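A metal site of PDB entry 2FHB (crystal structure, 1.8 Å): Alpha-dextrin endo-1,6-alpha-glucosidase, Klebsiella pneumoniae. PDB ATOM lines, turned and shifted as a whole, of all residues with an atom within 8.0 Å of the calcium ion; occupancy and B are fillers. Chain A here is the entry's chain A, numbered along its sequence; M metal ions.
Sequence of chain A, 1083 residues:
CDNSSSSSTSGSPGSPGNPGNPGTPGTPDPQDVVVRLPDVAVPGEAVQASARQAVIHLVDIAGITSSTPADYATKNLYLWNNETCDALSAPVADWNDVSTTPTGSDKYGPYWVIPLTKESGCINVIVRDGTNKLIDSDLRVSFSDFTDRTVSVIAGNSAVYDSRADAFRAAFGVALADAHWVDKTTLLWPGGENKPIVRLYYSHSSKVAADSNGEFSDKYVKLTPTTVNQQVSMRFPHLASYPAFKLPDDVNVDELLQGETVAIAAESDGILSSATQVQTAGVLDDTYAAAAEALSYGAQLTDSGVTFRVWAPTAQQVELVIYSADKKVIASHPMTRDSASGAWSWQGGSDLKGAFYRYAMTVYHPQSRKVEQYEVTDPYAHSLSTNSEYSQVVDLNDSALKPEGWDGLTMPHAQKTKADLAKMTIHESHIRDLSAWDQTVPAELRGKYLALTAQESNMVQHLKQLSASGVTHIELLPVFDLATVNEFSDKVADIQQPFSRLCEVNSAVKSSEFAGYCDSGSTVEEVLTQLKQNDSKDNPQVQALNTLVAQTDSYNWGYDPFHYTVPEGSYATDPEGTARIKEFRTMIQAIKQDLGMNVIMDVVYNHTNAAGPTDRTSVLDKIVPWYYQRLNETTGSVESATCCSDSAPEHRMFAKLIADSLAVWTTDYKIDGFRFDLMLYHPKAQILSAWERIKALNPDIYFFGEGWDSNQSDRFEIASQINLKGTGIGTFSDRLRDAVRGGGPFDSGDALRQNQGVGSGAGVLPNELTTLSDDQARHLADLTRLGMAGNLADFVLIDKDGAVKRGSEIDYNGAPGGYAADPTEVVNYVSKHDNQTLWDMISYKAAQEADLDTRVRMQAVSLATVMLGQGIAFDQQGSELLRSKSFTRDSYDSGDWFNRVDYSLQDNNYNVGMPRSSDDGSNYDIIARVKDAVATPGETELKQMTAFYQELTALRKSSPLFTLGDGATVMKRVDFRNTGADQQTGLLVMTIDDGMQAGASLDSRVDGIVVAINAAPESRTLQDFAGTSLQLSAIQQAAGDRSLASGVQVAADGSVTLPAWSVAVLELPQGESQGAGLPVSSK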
ATOM      1  N   GLU A  45      32.668  31.182  18.454  1.00  0.00           N
ATOM      2  CA  GLU A  45      33.076  29.782  18.525  1.00  0.00           C
ATOM      3  C   GLU A  45      34.501  29.638  18.039  1.00  0.00           C
ATOM      4  O   GLU A  45      34.801  29.875  16.876  1.00  0.00           O
ATOM      5  CB  GLU A  45      32.142  28.915  17.670  1.00  0.00           C
ATOM      6  CG  GLU A  45      30.707  28.886  18.167  1.00  0.00           C
ATOM      7  CD  GLU A  45      30.597  28.303  19.561  1.00  0.00           C
ATOM      8  OE1 GLU A  45      30.780  27.073  19.712  1.00  0.00           O
ATOM      9  OE2 GLU A  45      30.325  29.068  20.504  1.00  0.00           O
ATOM     10  N   VAL A  47      36.201  27.078  17.391  1.00  0.00           N
ATOM     11  CA  VAL A  47      36.244  26.129  16.279  1.00  0.00           C
ATOM     12  C   VAL A  47      35.106  25.110  16.372  1.00  0.00           C
ATOM     13  O   VAL A  47      34.632  24.785  17.459  1.00  0.00           O
ATOM     14  CB  VAL A  47      37.588  25.373  16.252  1.00  0.00           C
ATOM     15  CG1 VAL A  47      37.743  24.533  17.516  1.00  0.00           C
ATOM     16  CG2 VAL A  47      37.684  24.496  15.011  1.00  0.00           C
ATOM     17  N   GLN A  48      34.688  24.613  15.216  1.00  0.00           N
ATOM     18  CA  GLN A  48      33.617  23.617  15.161  1.00  0.00           C
ATOM     19  C   GLN A  48      34.215  22.241  14.925  1.00  0.00           C
ATOM     20  O   GLN A  48      35.347  22.112  14.461  1.00  0.00           O
ATOM     21  CB  GLN A  48      32.639  23.952  14.021  1.00  0.00           C
ATOM     22  CG  GLN A  48      31.904  25.272  14.205  1.00  0.00           C
ATOM     23  CD  GLN A  48      30.922  25.248  15.375  1.00  0.00           C
ATOM     24  OE1 GLN A  48      30.324  26.269  15.718  1.00  0.00           O
ATOM     25  NE2 GLN A  48      30.750  24.077  15.980  1.00  0.00           N
ATOM     26  N   ALA A  49      33.459  21.197  15.256  1.00  0.00           N
ATOM     27  CA  ALA A  49      33.926  19.825  15.088  1.00  0.00           C
ATOM     28  C   ALA A  49      33.804  19.380  13.631  1.00  0.00           C
ATOM     29  O   ALA A  49      32.912  19.817  12.913  1.00  0.00           O
ATOM     30  CB  ALA A  49      33.117  18.898  15.979  1.00  0.00           C
ATOM     31  N   VAL A  55      34.693  18.929  19.801  1.00  0.00           N
ATOM     32  CA  VAL A  55      35.330  20.105  20.366  1.00  0.00           C
ATOM     33  C   VAL A  55      34.627  20.551  21.642  1.00  0.00           C
ATOM     34  O   VAL A  55      33.395  20.518  21.722  1.00  0.00           O
ATOM     35  CB  VAL A  55      35.329  21.272  19.360  1.00  0.00           C
ATOM     36  CG1 VAL A  55      36.022  22.491  19.957  1.00  0.00           C
ATOM     37  CG2 VAL A  55      36.016  20.853  18.074  1.00  0.00           C
ATOM     38  N   HIS A  57      34.687  23.732  24.638  1.00  0.00           N
ATOM     39  CA  HIS A  57      35.172  25.044  25.043  1.00  0.00           C
ATOM     40  C   HIS A  57      35.052  25.260  26.553  1.00  0.00           C
ATOM     41  O   HIS A  57      34.138  24.745  27.196  1.00  0.00           O
ATOM     42  CB  HIS A  57      34.376  26.143  24.339  1.00  0.00           C
ATOM     43  CG  HIS A  57      34.406  26.058  22.851  1.00  0.00           C
ATOM     44  ND1 HIS A  57      35.549  26.266  22.101  1.00  0.00           N
ATOM     45  CD2 HIS A  57      33.418  25.803  21.951  1.00  0.00           C
ATOM     46  CE1 HIS A  57      35.275  26.133  20.821  1.00  0.00           C
ATOM     47  NE2 HIS A  57      33.989  25.864  20.701  1.00  0.00           N
ATOM     48  N   ASP A 145      21.899  15.537  21.452  1.00  0.00           N
ATOM     49  CA  ASP A 145      21.478  16.838  21.968  1.00  0.00           C
ATOM     50  C   ASP A 145      22.252  17.958  21.274  1.00  0.00           C
ATOM     51  O   ASP A 145      21.750  19.071  21.126  1.00  0.00           O
ATOM     52  CB  ASP A 145      21.709  16.906  23.477  1.00  0.00           C
ATOM     53  CG  ASP A 145      20.835  15.928  24.251  1.00  0.00           C
ATOM     54  OD1 ASP A 145      20.904  14.723  23.965  1.00  0.00           O
ATOM     55  OD2 ASP A 145      20.069  16.381  25.123  1.00  0.00           O
ATOM     56  N   PHE A 146      23.484  17.649  20.868  1.00  0.00           N
ATOM     57  CA  PHE A 146      24.325  18.620  20.179  1.00  0.00           C
ATOM     58  C   PHE A 146      24.861  17.987  18.903  1.00  0.00           C
ATOM     59  O   PHE A 146      25.957  17.418  18.887  1.00  0.00           O
ATOM     60  CB  PHE A 146      25.501  19.042  21.070  1.00  0.00           C
ATOM     61  CG  PHE A 146      25.089  19.482  22.445  1.00  0.00           C
ATOM     62  CD1 PHE A 146      24.791  18.543  23.431  1.00  0.00           C
ATOM     63  CD2 PHE A 146      24.995  20.833  22.760  1.00  0.00           C
ATOM     64  CE1 PHE A 146      24.398  18.946  24.710  1.00  0.00           C
ATOM     65  CE2 PHE A 146      24.603  21.248  24.033  1.00  0.00           C
ATOM     66  CZ  PHE A 146      24.304  20.299  25.010  1.00  0.00           C
ATOM     67  N   THR A 147      24.079  18.070  17.827  1.00  0.00           N
ATOM     68  CA  THR A 147      24.468  17.500  16.539  1.00  0.00           C
ATOM     69  C   THR A 147      25.816  18.030  16.058  1.00  0.00           C
ATOM     70  O   THR A 147      26.579  17.313  15.408  1.00  0.00           O
ATOM     71  CB  THR A 147      23.403  17.797  15.461  1.00  0.00           C
ATOM     72  OG1 THR A 147      23.809  17.196  14.227  1.00  0.00           O
ATOM     73  CG2 THR A 147      23.228  19.297  15.274  1.00  0.00           C
ATOM     74  N   ASP A 148      26.104  19.288  16.376  1.00  0.00           N
ATOM     75  CA  ASP A 148      27.361  19.919  15.972  1.00  0.00           C
ATOM     76  C   ASP A 148      28.529  19.406  16.805  1.00  0.00           C
ATOM     77  O   ASP A 148      29.691  19.649  16.477  1.00  0.00           O
ATOM     78  CB  ASP A 148      27.254  21.439  16.090  1.00  0.00           C
ATOM     79  CG  ASP A 148      26.855  21.884  17.480  1.00  0.00           C
ATOM     80  OD1 ASP A 148      27.592  21.573  18.442  1.00  0.00           O
ATOM     81  OD2 ASP A 148      25.803  22.550  17.612  1.00  0.00           O
ATOM     82  N   ARG A 149      28.212  18.706  17.886  1.00  0.00           N
ATOM     83  CA  ARG A 149      29.224  18.158  18.783  1.00  0.00           C
ATOM     84  C   ARG A 149      30.260  19.199  19.192  1.00  0.00           C
ATOM     85  O   ARG A 149      31.449  18.903  19.271  1.00  0.00           O
ATOM     86  CB  ARG A 149      29.919  16.962  18.116  1.00  0.00           C
ATOM     87  CG  ARG A 149      28.976  15.823  17.738  1.00  0.00           C
ATOM     88  CD  ARG A 149      29.731  14.630  17.169  1.00  0.00           C
ATOM     89  NE  ARG A 149      30.475  14.973  15.957  1.00  0.00           N
ATOM     90  CZ  ARG A 149      29.919  15.393  14.824  1.00  0.00           C
ATOM     91  NH1 ARG A 149      28.598  15.513  14.737  1.00  0.00           N
ATOM     92  NH2 ARG A 149      30.676  15.677  13.777  1.00  0.00           N
ATOM     93  N   THR A 150      29.787  20.413  19.458  1.00  0.00           N
ATOM     94  CA  THR A 150      30.665  21.508  19.869  1.00  0.00           C
ATOM     95  C   THR A 150      30.032  22.222  21.055  1.00  0.00           C
ATOM     96  O   THR A 150      29.271  23.175  20.890  1.00  0.00           O
ATOM     97  CB  THR A 150      30.864  22.522  18.715  1.00  0.00           C
ATOM     98  OG1 THR A 150      31.378  21.837  17.562  1.00  0.00           O
ATOM     99  CG2 THR A 150      31.845  23.611  19.122  1.00  0.00           C
ATOM    100  N   VAL A 151      30.363  21.770  22.268  1.00  0.00           N
ATOM    101  CA  VAL A 151      29.811  22.353  23.483  1.00  0.00           C
ATOM    102  C   VAL A 151      30.791  23.275  24.208  1.00  0.00           C
ATOM    103  O   VAL A 151      31.977  23.331  23.882  1.00  0.00           O
ATOM    104  CB  VAL A 151      29.375  21.247  24.462  1.00  0.00           C
ATOM    105  CG1 VAL A 151      28.296  20.383  23.824  1.00  0.00           C
ATOM    106  CG2 VAL A 151      30.564  20.392  24.870  1.00  0.00           C
ATOM    107  N   SER A 152      30.269  23.997  25.201  1.00  0.00           N
ATOM    108  CA  SER A 152      31.066  24.915  26.000  1.00  0.00           C
ATOM    109  C   SER A 152      30.682  24.781  27.467  1.00  0.00           C
ATOM    110  O   SER A 152      29.515  24.546  27.796  1.00  0.00           O
ATOM    111  CB  SER A 152      30.829  26.359  25.546  1.00  0.00           C
ATOM    112  OG  SER A 152      31.166  26.523  24.176  1.00  0.00           O
ATOM    113  N   TYR A 161      26.535  23.696  27.839  1.00  0.00           N
ATOM    114  CA  TYR A 161      25.939  24.586  26.846  1.00  0.00           C
ATOM    115  C   TYR A 161      26.338  24.239  25.417  1.00  0.00           C
ATOM    116  O   TYR A 161      27.327  23.545  25.184  1.00  0.00           O
ATOM    117  CB  TYR A 161      26.331  26.027  27.167  1.00  0.00           C
ATOM    118  CG  TYR A 161      25.861  26.466  28.536  1.00  0.00           C
ATOM    119  CD1 TYR A 161      24.523  26.726  28.790  1.00  0.00           C
ATOM    120  CD2 TYR A 161      26.764  26.566  29.600  1.00  0.00           C
ATOM    121  CE1 TYR A 161      24.069  27.080  30.058  1.00  0.00           C
ATOM    122  CE2 TYR A 161      26.327  26.918  30.881  1.00  0.00           C
ATOM    123  CZ  TYR A 161      24.982  27.178  31.100  1.00  0.00           C
ATOM    124  OH  TYR A 161      24.550  27.524  32.352  1.00  0.00           O
ATOM    125  N   ASP A 162      25.540  24.713  24.465  1.00  0.00           N
ATOM    126  CA  ASP A 162      25.770  24.449  23.048  1.00  0.00           C
ATOM    127  C   ASP A 162      26.790  25.396  22.410  1.00  0.00           C
ATOM    128  O   ASP A 162      27.408  25.057  21.396  1.00  0.00           O
ATOM    129  CB  ASP A 162      24.445  24.512  22.287  1.00  0.00           C
ATOM    130  CG  ASP A 162      24.579  24.097  20.835  1.00  0.00           C
ATOM    131  OD1 ASP A 162      25.230  24.829  20.062  1.00  0.00           O
ATOM    132  OD2 ASP A 162      24.034  23.039  20.471  1.00  0.00           O
ATOM    133  N   SER A 163      26.965  26.564  22.999  1.00  0.00           N
ATOM    134  CA  SER A 163      27.920  27.542  22.472  1.00  0.00           C
ATOM    135  C   SER A 163      28.558  28.360  23.584  1.00  0.00           C
ATOM    136  O   SER A 163      28.042  28.408  24.702  1.00  0.00           O
ATOM    137  CB  SER A 163      27.223  28.486  21.486  1.00  0.00           C
ATOM    138  OG  SER A 163      26.245  29.282  22.135  1.00  0.00           O
ATOM    139  N   ARG A 164      29.679  29.002  23.276  1.00  0.00           N
ATOM    140  CA  ARG A 164      30.378  29.824  24.267  1.00  0.00           C
ATOM    141  C   ARG A 164      29.543  31.054  24.586  1.00  0.00           C
ATOM    142  O   ARG A 164      29.675  31.643  25.658  1.00  0.00           O
ATOM    143  CB  ARG A 164      31.753  30.246  23.739  1.00  0.00           C
ATOM    144  CG  ARG A 164      32.684  29.074  23.438  1.00  0.00           C
ATOM    145  CD  ARG A 164      34.148  29.512  23.365  1.00  0.00           C
ATOM    146  NE  ARG A 164      34.400  30.489  22.306  1.00  0.00           N
ATOM    147  CZ  ARG A 164      35.591  31.015  22.041  1.00  0.00           C
ATOM    148  NH1 ARG A 164      36.649  30.661  22.751  1.00  0.00           N
ATOM    149  NH2 ARG A 164      35.719  31.905  21.068  1.00  0.00           N
ATOM    150  N   ASP A 166      26.230  31.059  24.871  1.00  0.00           N
ATOM    151  CA  ASP A 166      25.237  30.624  25.837  1.00  0.00           C
ATOM    152  C   ASP A 166      25.841  30.500  27.234  1.00  0.00           C
ATOM    153  O   ASP A 166      25.295  31.020  28.207  1.00  0.00           O
ATOM    154  CB  ASP A 166      24.634  29.275  25.424  1.00  0.00           C
ATOM    155  CG  ASP A 166      23.772  29.375  24.174  1.00  0.00           C
ATOM    156  OD1 ASP A 166      23.278  28.325  23.710  1.00  0.00           O
ATOM    157  OD2 ASP A 166      23.585  30.500  23.672  1.00  0.00           O
HETATM  158 CA    CA M   1      27.630  23.885  19.262  1.00  0.00          CA
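The nearest printed residue that does not touch the calcium ion is Glu 45 (4.5 Å).
OG1 of Thr 150 sits at hydrogen-bond distance from N of Ala 49. The side-chain hydroxyl (OG1) of Thr 150 lies within hydrogen-bond range of the side-chain amide nitrogen (NE2) of Gln 48 (2.8 Å).
The calcium ion is bound by O of Thr 150 (2.4 Å), O of Asp 162 (2.4 Å), OD1 of Asp 148 (2.5 Å), OD1 of Asp 162 (2.7 Å) and OD2 of Asp 148 (2.8 Å).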
